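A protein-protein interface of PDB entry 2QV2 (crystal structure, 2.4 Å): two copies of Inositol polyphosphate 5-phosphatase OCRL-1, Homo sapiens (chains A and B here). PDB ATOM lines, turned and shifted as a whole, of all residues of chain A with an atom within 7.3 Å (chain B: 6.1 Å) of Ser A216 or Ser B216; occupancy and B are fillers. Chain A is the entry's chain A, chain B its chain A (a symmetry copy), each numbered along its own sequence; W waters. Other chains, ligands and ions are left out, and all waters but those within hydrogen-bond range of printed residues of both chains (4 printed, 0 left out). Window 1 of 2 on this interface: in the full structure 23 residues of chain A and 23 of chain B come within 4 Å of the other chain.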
ATOM      1  N   ARG A 133      -8.669  -9.303  22.630  1.00  0.00           N
ATOM      2  CA  ARG A 133      -7.613 -10.305  22.595  1.00  0.00           C
ATOM      3  C   ARG A 133      -6.529  -9.990  23.632  1.00  0.00           C
ATOM      4  O   ARG A 133      -6.445  -8.873  24.141  1.00  0.00           O
ATOM      5  CB  ARG A 133      -6.956 -10.324  21.212  1.00  0.00           C
ATOM      6  CG  ARG A 133      -7.895 -10.551  20.032  1.00  0.00           C
ATOM      7  CD  ARG A 133      -8.070 -12.030  19.712  1.00  0.00           C
ATOM      8  NE  ARG A 133      -9.186 -12.635  20.434  1.00  0.00           N
ATOM      9  CZ  ARG A 133      -9.133 -13.818  21.043  1.00  0.00           C
ATOM     10  NH1 ARG A 133     -10.200 -14.292  21.674  1.00  0.00           N
ATOM     11  NH2 ARG A 133      -8.006 -14.521  21.037  1.00  0.00           N
ATOM     12  N   PRO A 134      -5.691 -10.979  23.966  1.00  0.00           N
ATOM     13  CA  PRO A 134      -4.638 -10.696  24.940  1.00  0.00           C
ATOM     14  C   PRO A 134      -3.816  -9.540  24.378  1.00  0.00           C
ATOM     15  O   PRO A 134      -3.831  -9.308  23.172  1.00  0.00           O
ATOM     16  CB  PRO A 134      -3.861 -12.006  24.985  1.00  0.00           C
ATOM     17  CG  PRO A 134      -4.957 -13.023  24.818  1.00  0.00           C
ATOM     18  CD  PRO A 134      -5.774 -12.425  23.685  1.00  0.00           C
ATOM     19  N   ILE A 135      -3.112  -8.820  25.244  1.00  0.00           N
ATOM     20  CA  ILE A 135      -2.306  -7.680  24.834  1.00  0.00           C
ATOM     21  C   ILE A 135      -1.111  -8.082  23.983  1.00  0.00           C
ATOM     22  O   ILE A 135      -0.537  -7.264  23.263  1.00  0.00           O
ATOM     23  CB  ILE A 135      -1.823  -6.887  26.081  1.00  0.00           C
ATOM     24  CG1 ILE A 135      -1.144  -5.583  25.652  1.00  0.00           C
ATOM     25  CG2 ILE A 135      -0.875  -7.753  26.920  1.00  0.00           C
ATOM     26  CD1 ILE A 135      -0.996  -4.587  26.776  1.00  0.00           C
ATOM     27  N   ARG A 136      -0.741  -9.354  24.062  1.00  0.00           N
ATOM     28  CA  ARG A 136       0.392  -9.860  23.303  1.00  0.00           C
ATOM     29  C   ARG A 136       0.035 -11.148  22.583  1.00  0.00           C
ATOM     30  O   ARG A 136       0.889 -12.024  22.427  1.00  0.00           O
ATOM     31  CB  ARG A 136       1.580 -10.116  24.244  1.00  0.00           C
ATOM     32  CG  ARG A 136       2.573  -8.979  24.321  1.00  0.00           C
ATOM     33  CD  ARG A 136       3.329  -8.977  25.633  1.00  0.00           C
ATOM     34  NE  ARG A 136       3.892 -10.279  25.982  1.00  0.00           N
ATOM     35  CZ  ARG A 136       4.081 -10.675  27.240  1.00  0.00           C
ATOM     36  NH1 ARG A 136       3.751  -9.862  28.236  1.00  0.00           N
ATOM     37  NH2 ARG A 136       4.575 -11.874  27.511  1.00  0.00           N
ATOM     38  N   GLU A 137      -1.213 -11.290  22.146  1.00  0.00           N
ATOM     39  CA  GLU A 137      -1.554 -12.527  21.459  1.00  0.00           C
ATOM     40  C   GLU A 137      -0.814 -12.614  20.135  1.00  0.00           C
ATOM     41  O   GLU A 137      -0.613 -11.616  19.442  1.00  0.00           O
ATOM     42  CB  GLU A 137      -3.063 -12.697  21.222  1.00  0.00           C
ATOM     43  CG  GLU A 137      -3.378 -14.116  20.679  1.00  0.00           C
ATOM     44  CD  GLU A 137      -4.861 -14.422  20.517  1.00  0.00           C
ATOM     45  OE1 GLU A 137      -5.550 -13.719  19.738  1.00  0.00           O
ATOM     46  OE2 GLU A 137      -5.337 -15.378  21.169  1.00  0.00           O
ATOM     47  N   LYS A 177     -11.317  -8.511  30.361  1.00  0.00           N
ATOM     48  CA  LYS A 177     -11.353  -9.955  30.459  1.00  0.00           C
ATOM     49  C   LYS A 177     -10.345 -10.410  31.526  1.00  0.00           C
ATOM     50  O   LYS A 177     -10.606 -11.352  32.274  1.00  0.00           O
ATOM     51  CB  LYS A 177     -11.033 -10.594  29.097  1.00  0.00           C
ATOM     52  CG  LYS A 177      -9.726 -10.155  28.466  1.00  0.00           C
ATOM     53  CD  LYS A 177      -9.655 -10.646  27.018  1.00  0.00           C
ATOM     54  CE  LYS A 177      -8.285 -10.380  26.405  1.00  0.00           C
ATOM     55  NZ  LYS A 177      -8.000  -8.917  26.393  1.00  0.00           N
ATOM     56  N   GLU A 178      -9.207  -9.725  31.607  1.00  0.00           N
ATOM     57  CA  GLU A 178      -8.185 -10.096  32.581  1.00  0.00           C
ATOM     58  C   GLU A 178      -8.688 -10.084  34.027  1.00  0.00           C
ATOM     59  O   GLU A 178      -8.438 -11.033  34.778  1.00  0.00           O
ATOM     60  CB  GLU A 178      -6.971  -9.186  32.468  1.00  0.00           C
ATOM     61  CG  GLU A 178      -6.255  -9.270  31.139  1.00  0.00           C
ATOM     62  CD  GLU A 178      -6.988  -8.533  30.036  1.00  0.00           C
ATOM     63  OE1 GLU A 178      -7.643  -7.507  30.333  1.00  0.00           O
ATOM     64  OE2 GLU A 178      -6.892  -8.968  28.872  1.00  0.00           O
ATOM     65  N   LEU A 181     -11.249 -12.941  34.367  1.00  0.00           N
ATOM     66  CA  LEU A 181     -10.647 -14.266  34.477  1.00  0.00           C
ATOM     67  C   LEU A 181     -10.143 -14.527  35.893  1.00  0.00           C
ATOM     68  O   LEU A 181     -10.261 -15.639  36.406  1.00  0.00           O
ATOM     69  CB  LEU A 181      -9.481 -14.402  33.486  1.00  0.00           C
ATOM     70  CG  LEU A 181      -9.920 -14.547  32.023  1.00  0.00           C
ATOM     71  CD1 LEU A 181      -8.745 -14.297  31.075  1.00  0.00           C
ATOM     72  CD2 LEU A 181     -10.506 -15.930  31.829  1.00  0.00           C
ATOM     73  N   ILE A 210       0.665 -13.896  35.372  1.00  0.00           N
ATOM     74  CA  ILE A 210       0.822 -12.678  34.597  1.00  0.00           C
ATOM     75  C   ILE A 210       1.039 -13.022  33.118  1.00  0.00           C
ATOM     76  O   ILE A 210       0.317 -12.537  32.256  1.00  0.00           O
ATOM     77  CB  ILE A 210       2.004 -11.825  35.150  1.00  0.00           C
ATOM     78  CG1 ILE A 210       1.587 -11.183  36.480  1.00  0.00           C
ATOM     79  CG2 ILE A 210       2.390 -10.751  34.169  1.00  0.00           C
ATOM     80  CD1 ILE A 210       2.738 -10.658  37.334  1.00  0.00           C
ATOM     81  N   ASP A 211       2.014 -13.870  32.822  1.00  0.00           N
ATOM     82  CA  ASP A 211       2.274 -14.241  31.438  1.00  0.00           C
ATOM     83  C   ASP A 211       1.049 -14.876  30.798  1.00  0.00           C
ATOM     84  O   ASP A 211       0.784 -14.714  29.606  1.00  0.00           O
ATOM     85  CB  ASP A 211       3.454 -15.202  31.362  1.00  0.00           C
ATOM     86  CG  ASP A 211       4.672 -14.560  30.758  1.00  0.00           C
ATOM     87  OD1 ASP A 211       5.737 -15.209  30.726  1.00  0.00           O
ATOM     88  OD2 ASP A 211       4.562 -13.401  30.306  1.00  0.00           O
ATOM     89  N   CYS A 212       0.305 -15.609  31.606  1.00  0.00           N
ATOM     90  CA  CYS A 212      -0.896 -16.264  31.148  1.00  0.00           C
ATOM     91  C   CYS A 212      -1.908 -15.219  30.659  1.00  0.00           C
ATOM     92  O   CYS A 212      -2.381 -15.290  29.523  1.00  0.00           O
ATOM     93  CB  CYS A 212      -1.470 -17.083  32.305  1.00  0.00           C
ATOM     94  SG  CYS A 212      -3.052 -17.847  32.013  1.00  0.00           S
ATOM     95  N   LEU A 213      -2.235 -14.247  31.507  1.00  0.00           N
ATOM     96  CA  LEU A 213      -3.203 -13.210  31.148  1.00  0.00           C
ATOM     97  C   LEU A 213      -2.748 -12.305  30.006  1.00  0.00           C
ATOM     98  O   LEU A 213      -3.574 -11.732  29.287  1.00  0.00           O
ATOM     99  CB  LEU A 213      -3.523 -12.330  32.361  1.00  0.00           C
ATOM    100  CG  LEU A 213      -4.070 -13.043  33.597  1.00  0.00           C
ATOM    101  CD1 LEU A 213      -4.372 -12.021  34.672  1.00  0.00           C
ATOM    102  CD2 LEU A 213      -5.317 -13.810  33.250  1.00  0.00           C
ATOM    103  N   ASP A 214      -1.437 -12.164  29.844  1.00  0.00           N
ATOM    104  CA  ASP A 214      -0.897 -11.303  28.801  1.00  0.00           C
ATOM    105  C   ASP A 214      -0.907 -11.920  27.407  1.00  0.00           C
ATOM    106  O   ASP A 214      -0.872 -11.200  26.408  1.00  0.00           O
ATOM    107  CB  ASP A 214       0.548 -10.905  29.134  1.00  0.00           C
ATOM    108  CG  ASP A 214       0.643  -9.941  30.299  1.00  0.00           C
ATOM    109  OD1 ASP A 214      -0.390  -9.328  30.650  1.00  0.00           O
ATOM    110  OD2 ASP A 214       1.760  -9.784  30.848  1.00  0.00           O
ATOM    111  N   THR A 215      -0.977 -13.248  27.352  1.00  0.00           N
ATOM    112  CA  THR A 215      -0.897 -13.976  26.096  1.00  0.00           C
ATOM    113  C   THR A 215      -2.056 -14.874  25.734  1.00  0.00           C
ATOM    114  O   THR A 215      -2.102 -15.386  24.627  1.00  0.00           O
ATOM    115  CB  THR A 215       0.349 -14.870  26.088  1.00  0.00           C
ATOM    116  OG1 THR A 215       0.204 -15.875  27.096  1.00  0.00           O
ATOM    117  CG2 THR A 215       1.597 -14.058  26.387  1.00  0.00           C
ATOM    118  N   SER A 216      -2.992 -15.087  26.645  1.00  0.00           N
ATOM    119  CA  SER A 216      -4.088 -15.978  26.332  1.00  0.00           C
ATOM    120  C   SER A 216      -5.294 -15.666  27.172  1.00  0.00           C
ATOM    121  O   SER A 216      -5.215 -14.882  28.100  1.00  0.00           O
ATOM    122  CB  SER A 216      -3.658 -17.416  26.608  1.00  0.00           C
ATOM    123  OG  SER A 216      -3.411 -17.611  27.996  1.00  0.00           O
ATOM    124  N   ILE A 217      -6.419 -16.273  26.819  1.00  0.00           N
ATOM    125  CA  ILE A 217      -7.639 -16.132  27.590  1.00  0.00           C
ATOM    126  C   ILE A 217      -7.754 -17.552  28.113  1.00  0.00           C
ATOM    127  O   ILE A 217      -8.564 -18.336  27.635  1.00  0.00           O
ATOM    128  CB  ILE A 217      -8.857 -15.819  26.713  1.00  0.00           C
ATOM    129  CG1 ILE A 217      -8.557 -14.610  25.822  1.00  0.00           C
ATOM    130  CG2 ILE A 217     -10.081 -15.554  27.608  1.00  0.00           C
ATOM    131  CD1 ILE A 217      -9.712 -14.217  24.910  1.00  0.00           C
ATOM    132  N   PRO A 218      -6.924 -17.901  29.107  1.00  0.00           N
ATOM    133  CA  PRO A 218      -6.885 -19.235  29.715  1.00  0.00           C
ATOM    134  C   PRO A 218      -8.190 -19.877  30.136  1.00  0.00           C
ATOM    135  O   PRO A 218      -9.115 -19.219  30.623  1.00  0.00           O
ATOM    136  CB  PRO A 218      -5.925 -19.051  30.887  1.00  0.00           C
ATOM    137  CG  PRO A 218      -6.145 -17.621  31.273  1.00  0.00           C
ATOM    138  CD  PRO A 218      -6.189 -16.931  29.941  1.00  0.00           C
ATOM    139  N   GLU A 219      -8.242 -21.185  29.934  1.00  0.00           N
ATOM    140  CA  GLU A 219      -9.386 -22.004  30.293  1.00  0.00           C
ATOM    141  C   GLU A 219      -9.265 -22.250  31.797  1.00  0.00           C
ATOM    142  O   GLU A 219     -10.257 -22.442  32.499  1.00  0.00           O
ATOM    143  CB  GLU A 219      -9.314 -23.314  29.508  1.00  0.00           C
ATOM    144  CG  GLU A 219     -10.292 -24.403  29.922  1.00  0.00           C
ATOM    145  CD  GLU A 219     -10.082 -25.687  29.131  1.00  0.00           C
ATOM    146  OE1 GLU A 219     -10.830 -25.936  28.163  1.00  0.00           O
ATOM    147  OE2 GLU A 219      -9.148 -26.441  29.477  1.00  0.00           O
ATOM    148  N   THR A 220      -8.032 -22.214  32.283  1.00  0.00           N
ATOM    149  CA  THR A 220      -7.745 -22.423  33.692  1.00  0.00           C
ATOM    150  C   THR A 220      -6.504 -21.623  34.075  1.00  0.00           C
ATOM    151  O   THR A 220      -5.416 -21.855  33.540  1.00  0.00           O
ATOM    152  CB  THR A 220      -7.460 -23.914  34.002  1.00  0.00           C
ATOM    153  OG1 THR A 220      -8.639 -24.695  33.779  1.00  0.00           O
ATOM    154  CG2 THR A 220      -7.022 -24.087  35.449  1.00  0.00           C
ATOM    155  N   ILE A 221      -6.665 -20.670  34.987  1.00  0.00           N
ATOM    156  CA  ILE A 221      -5.530 -19.885  35.444  1.00  0.00           C
ATOM    157  C   ILE A 221      -4.671 -20.842  36.268  1.00  0.00           C
ATOM    158  O   ILE A 221      -5.176 -21.543  37.144  1.00  0.00           O
ATOM    159  CB  ILE A 221      -5.962 -18.732  36.372  1.00  0.00           C
ATOM    160  CG1 ILE A 221      -6.920 -17.783  35.647  1.00  0.00           C
ATOM    161  CG2 ILE A 221      -4.733 -17.982  36.853  1.00  0.00           C
ATOM    162  CD1 ILE A 221      -6.297 -17.058  34.495  1.00  0.00           C
ATOM    163  N   PRO B 134      -8.318 -20.997  19.078  1.00  0.00           N
ATOM    164  CA  PRO B 134      -8.103 -22.345  19.603  1.00  0.00           C
ATOM    165  C   PRO B 134      -9.450 -23.059  19.545  1.00  0.00           C
ATOM    166  O   PRO B 134     -10.489 -22.407  19.502  1.00  0.00           O
ATOM    167  CB  PRO B 134      -7.638 -22.078  21.030  1.00  0.00           C
ATOM    168  CG  PRO B 134      -6.825 -20.824  20.862  1.00  0.00           C
ATOM    169  CD  PRO B 134      -7.719 -19.984  19.967  1.00  0.00           C
ATOM    170  N   GLU B 137     -11.133 -22.084  22.867  1.00  0.00           N
ATOM    171  CA  GLU B 137     -10.866 -20.783  23.466  1.00  0.00           C
ATOM    172  C   GLU B 137     -12.091 -20.289  24.214  1.00  0.00           C
ATOM    173  O   GLU B 137     -13.231 -20.499  23.796  1.00  0.00           O
ATOM    174  CB  GLU B 137     -10.417 -19.723  22.448  1.00  0.00           C
ATOM    175  CG  GLU B 137      -9.951 -18.431  23.169  1.00  0.00           C
ATOM    176  CD  GLU B 137      -9.380 -17.359  22.251  1.00  0.00           C
ATOM    177  OE1 GLU B 137     -10.109 -16.871  21.352  1.00  0.00           O
ATOM    178  OE2 GLU B 137      -8.197 -16.997  22.436  1.00  0.00           O
ATOM    179  N   LYS B 177      -2.773 -23.397  12.586  1.00  0.00           N
ATOM    180  CA  LYS B 177      -1.905 -22.652  13.473  1.00  0.00           C
ATOM    181  C   LYS B 177      -1.204 -23.632  14.428  1.00  0.00           C
ATOM    182  O   LYS B 177      -0.033 -23.455  14.759  1.00  0.00           O
ATOM    183  CB  LYS B 177      -2.711 -21.604  14.258  1.00  0.00           C
ATOM    184  CG  LYS B 177      -3.896 -22.146  15.035  1.00  0.00           C
ATOM    185  CD  LYS B 177      -4.759 -20.990  15.546  1.00  0.00           C
ATOM    186  CE  LYS B 177      -5.858 -21.484  16.478  1.00  0.00           C
ATOM    187  NZ  LYS B 177      -6.760 -22.429  15.760  1.00  0.00           N
ATOM    188  N   LEU B 181       2.651 -23.580  15.083  1.00  0.00           N
ATOM    189  CA  LEU B 181       3.235 -23.252  16.379  1.00  0.00           C
ATOM    190  C   LEU B 181       4.276 -24.289  16.792  1.00  0.00           C
ATOM    191  O   LEU B 181       5.310 -23.946  17.363  1.00  0.00           O
ATOM    192  CB  LEU B 181       2.139 -23.174  17.451  1.00  0.00           C
ATOM    193  CG  LEU B 181       1.258 -21.921  17.352  1.00  0.00           C
ATOM    194  CD1 LEU B 181      -0.017 -22.086  18.180  1.00  0.00           C
ATOM    195  CD2 LEU B 181       2.067 -20.725  17.810  1.00  0.00           C
ATOM    196  N   ASP B 211      -2.752 -29.253  25.934  1.00  0.00           N
ATOM    197  CA  ASP B 211      -3.699 -28.306  26.506  1.00  0.00           C
ATOM    198  C   ASP B 211      -3.407 -26.887  26.041  1.00  0.00           C
ATOM    199  O   ASP B 211      -4.309 -26.069  25.851  1.00  0.00           O
ATOM    200  CB  ASP B 211      -3.659 -28.370  28.027  1.00  0.00           C
ATOM    201  CG  ASP B 211      -4.901 -28.992  28.603  1.00  0.00           C
ATOM    202  OD1 ASP B 211      -4.953 -29.193  29.834  1.00  0.00           O
ATOM    203  OD2 ASP B 211      -5.832 -29.276  27.822  1.00  0.00           O
ATOM    204  N   CYS B 212      -2.130 -26.602  25.863  1.00  0.00           N
ATOM    205  CA  CYS B 212      -1.696 -25.302  25.413  1.00  0.00           C
ATOM    206  C   CYS B 212      -2.274 -25.012  24.020  1.00  0.00           C
ATOM    207  O   CYS B 212      -2.932 -23.990  23.816  1.00  0.00           O
ATOM    208  CB  CYS B 212      -0.168 -25.285  25.387  1.00  0.00           C
ATOM    209  SG  CYS B 212       0.587 -23.826  24.698  1.00  0.00           S
ATOM    210  N   LEU B 213      -2.037 -25.909  23.067  1.00  0.00           N
ATOM    211  CA  LEU B 213      -2.526 -25.722  21.700  1.00  0.00           C
ATOM    212  C   LEU B 213      -4.048 -25.731  21.579  1.00  0.00           C
ATOM    213  O   LEU B 213      -4.610 -25.137  20.653  1.00  0.00           O
ATOM    214  CB  LEU B 213      -1.963 -26.806  20.775  1.00  0.00           C
ATOM    215  CG  LEU B 213      -0.441 -26.912  20.694  1.00  0.00           C
ATOM    216  CD1 LEU B 213      -0.066 -27.995  19.705  1.00  0.00           C
ATOM    217  CD2 LEU B 213       0.154 -25.598  20.268  1.00  0.00           C
ATOM    218  N   ASP B 214      -4.714 -26.413  22.504  1.00  0.00           N
ATOM    219  CA  ASP B 214      -6.166 -26.507  22.466  1.00  0.00           C
ATOM    220  C   ASP B 214      -6.892 -25.273  22.989  1.00  0.00           C
ATOM    221  O   ASP B 214      -8.055 -25.045  22.653  1.00  0.00           O
ATOM    222  CB  ASP B 214      -6.643 -27.718  23.280  1.00  0.00           C
ATOM    223  CG  ASP B 214      -6.311 -29.042  22.621  1.00  0.00           C
ATOM    224  OD1 ASP B 214      -6.006 -29.043  21.407  1.00  0.00           O
ATOM    225  OD2 ASP B 214      -6.375 -30.083  23.318  1.00  0.00           O
ATOM    226  N   THR B 215      -6.191 -24.474  23.791  1.00  0.00           N
ATOM    227  CA  THR B 215      -6.783 -23.316  24.441  1.00  0.00           C
ATOM    228  C   THR B 215      -6.161 -21.967  24.168  1.00  0.00           C
ATOM    229  O   THR B 215      -6.711 -20.954  24.569  1.00  0.00           O
ATOM    230  CB  THR B 215      -6.751 -23.497  25.964  1.00  0.00           C
ATOM    231  OG1 THR B 215      -5.387 -23.515  26.399  1.00  0.00           O
ATOM    232  CG2 THR B 215      -7.407 -24.806  26.365  1.00  0.00           C
ATOM    233  N   SER B 216      -5.018 -21.929  23.502  1.00  0.00           N
ATOM    234  CA  SER B 216      -4.383 -20.649  23.268  1.00  0.00           C
ATOM    235  C   SER B 216      -3.482 -20.705  22.067  1.00  0.00           C
ATOM    236  O   SER B 216      -3.227 -21.771  21.534  1.00  0.00           O
ATOM    237  CB  SER B 216      -3.549 -20.274  24.489  1.00  0.00           C
ATOM    238  OG  SER B 216      -2.474 -21.189  24.667  1.00  0.00           O
ATOM    239  N   ILE B 217      -3.022 -19.540  21.632  1.00  0.00           N
ATOM    240  CA  ILE B 217      -2.076 -19.451  20.537  1.00  0.00           C
ATOM    241  C   ILE B 217      -0.870 -18.949  21.308  1.00  0.00           C
ATOM    242  O   ILE B 217      -0.521 -17.777  21.239  1.00  0.00           O
ATOM    243  CB  ILE B 217      -2.480 -18.401  19.494  1.00  0.00           C
ATOM    244  CG1 ILE B 217      -3.918 -18.654  19.036  1.00  0.00           C
ATOM    245  CG2 ILE B 217      -1.505 -18.458  18.305  1.00  0.00           C
ATOM    246  CD1 ILE B 217      -4.415 -17.660  17.993  1.00  0.00           C
ATOM    247  N   PRO B 218      -0.217 -19.843  22.067  1.00  0.00           N
ATOM    248  CA  PRO B 218       0.953 -19.526  22.891  1.00  0.00           C
ATOM    249  C   PRO B 218       2.085 -18.739  22.267  1.00  0.00           C
ATOM    250  O   PRO B 218       2.430 -18.910  21.094  1.00  0.00           O
ATOM    251  CB  PRO B 218       1.404 -20.894  23.390  1.00  0.00           C
ATOM    252  CG  PRO B 218       1.003 -21.803  22.269  1.00  0.00           C
ATOM    253  CD  PRO B 218      -0.369 -21.304  21.924  1.00  0.00           C
HETATM  254  O   HOH W   1      -8.998 -19.884  25.726  1.00  0.00           O
HETATM  255  O   HOH W   2      -3.834 -17.233  23.014  1.00  0.00           O
HETATM  256  O   HOH W   3      -0.984 -15.475  22.085  1.00  0.00           O
HETATM  257  O   HOH W   4      -6.324 -17.977  24.589  1.00  0.00           O
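Along chain A the printed residues that touch a printed residue of chain B span positions 133 to 219. Among the printed residues, 4 pairs touch across the chains. Among the printed residues, Asp or Glu carboxylates within 4 Å of a Lys or Arg side-chain nitrogen of the other chain: Arg A133 with Glu B137.
Of chain B, only Ser B216 (3.6 Å) comes within 4 Å of Ser A216. Of the printed residues of chain A, Ser B216 touches Ser A216 (3.6 Å). Of the printed residues of chain A, Glu B137 touches Arg A133 and Glu A137. Of the printed residues of chain B, Glu A137 touches Glu B137 (3.5 Å). Glu A178 touches none of the printed residues of chain B. The nearest residue of chain B that does not touch Ser A216 is Thr B215 (5.1 Å). The nearest residue of chain A that does not touch Ser B216 is Thr A215 (5.1 Å). The nearest printed residue of chain B that does not touch Glu A219 is Asp B211 (4.7 Å).
Water W1 bridges O of Ile A217 (2.5 Å) and O of Thr B215 (2.8 Å). Water W3 bridges the backbone carbonyl oxygen (O) of Ile B217 (2.5 Å) and the backbone carbonyl oxygen (O) of Thr A215 (2.8 Å). Water W4 lies within hydrogen-bond range of the backbone NH (N) of Ile A217 (2.8 Å), the backbone carbonyl oxygen (O) of Thr B215 (3.0 Å) and the side-chain carboxylate (OE2) of Glu B137 (3.0 Å). Water W2 lies within hydrogen-bond range of N of Ile B217 (2.8 Å), O of Thr A215 (3.0 Å) and OE2 of Glu A137 (3.0 Å).
The guanidinium group of Arg A133 is in salt-bridge range of the side-chain carboxylate of Glu A137. O of Arg A133 is in hydrogen-bond range of NZ of Lys A177 (2.7 Å). O of Cys A212 is in hydrogen-bond range of OG of Ser A216. The backbone carbonyl oxygen of Asp B211 sits at hydrogen-bond distance from the side-chain hydroxyl of Thr B215 (2.8 Å). The side-chain hydroxyl of Ser B216 sits at hydrogen-bond distance from the backbone carbonyl oxygen of Cys B212.
Glu A137 touches its own counterpart, Glu B137. Ser B216 touches its own counterpart, Ser A216. 12 positions are printed for both chains. Of the 4 pairs that touch across the chains among the printed residues, 2 have their exchanged pair printed and touching as well.
Among the printed residues, merely in contact across the chains: Glu A137 with Glu B137, Ser A216 with Ser B216 and Glu A219 with Thr B215.
The guanidinium group of Arg A133 lies within salt-bridge range of the side-chain carboxylate of Glu B137.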
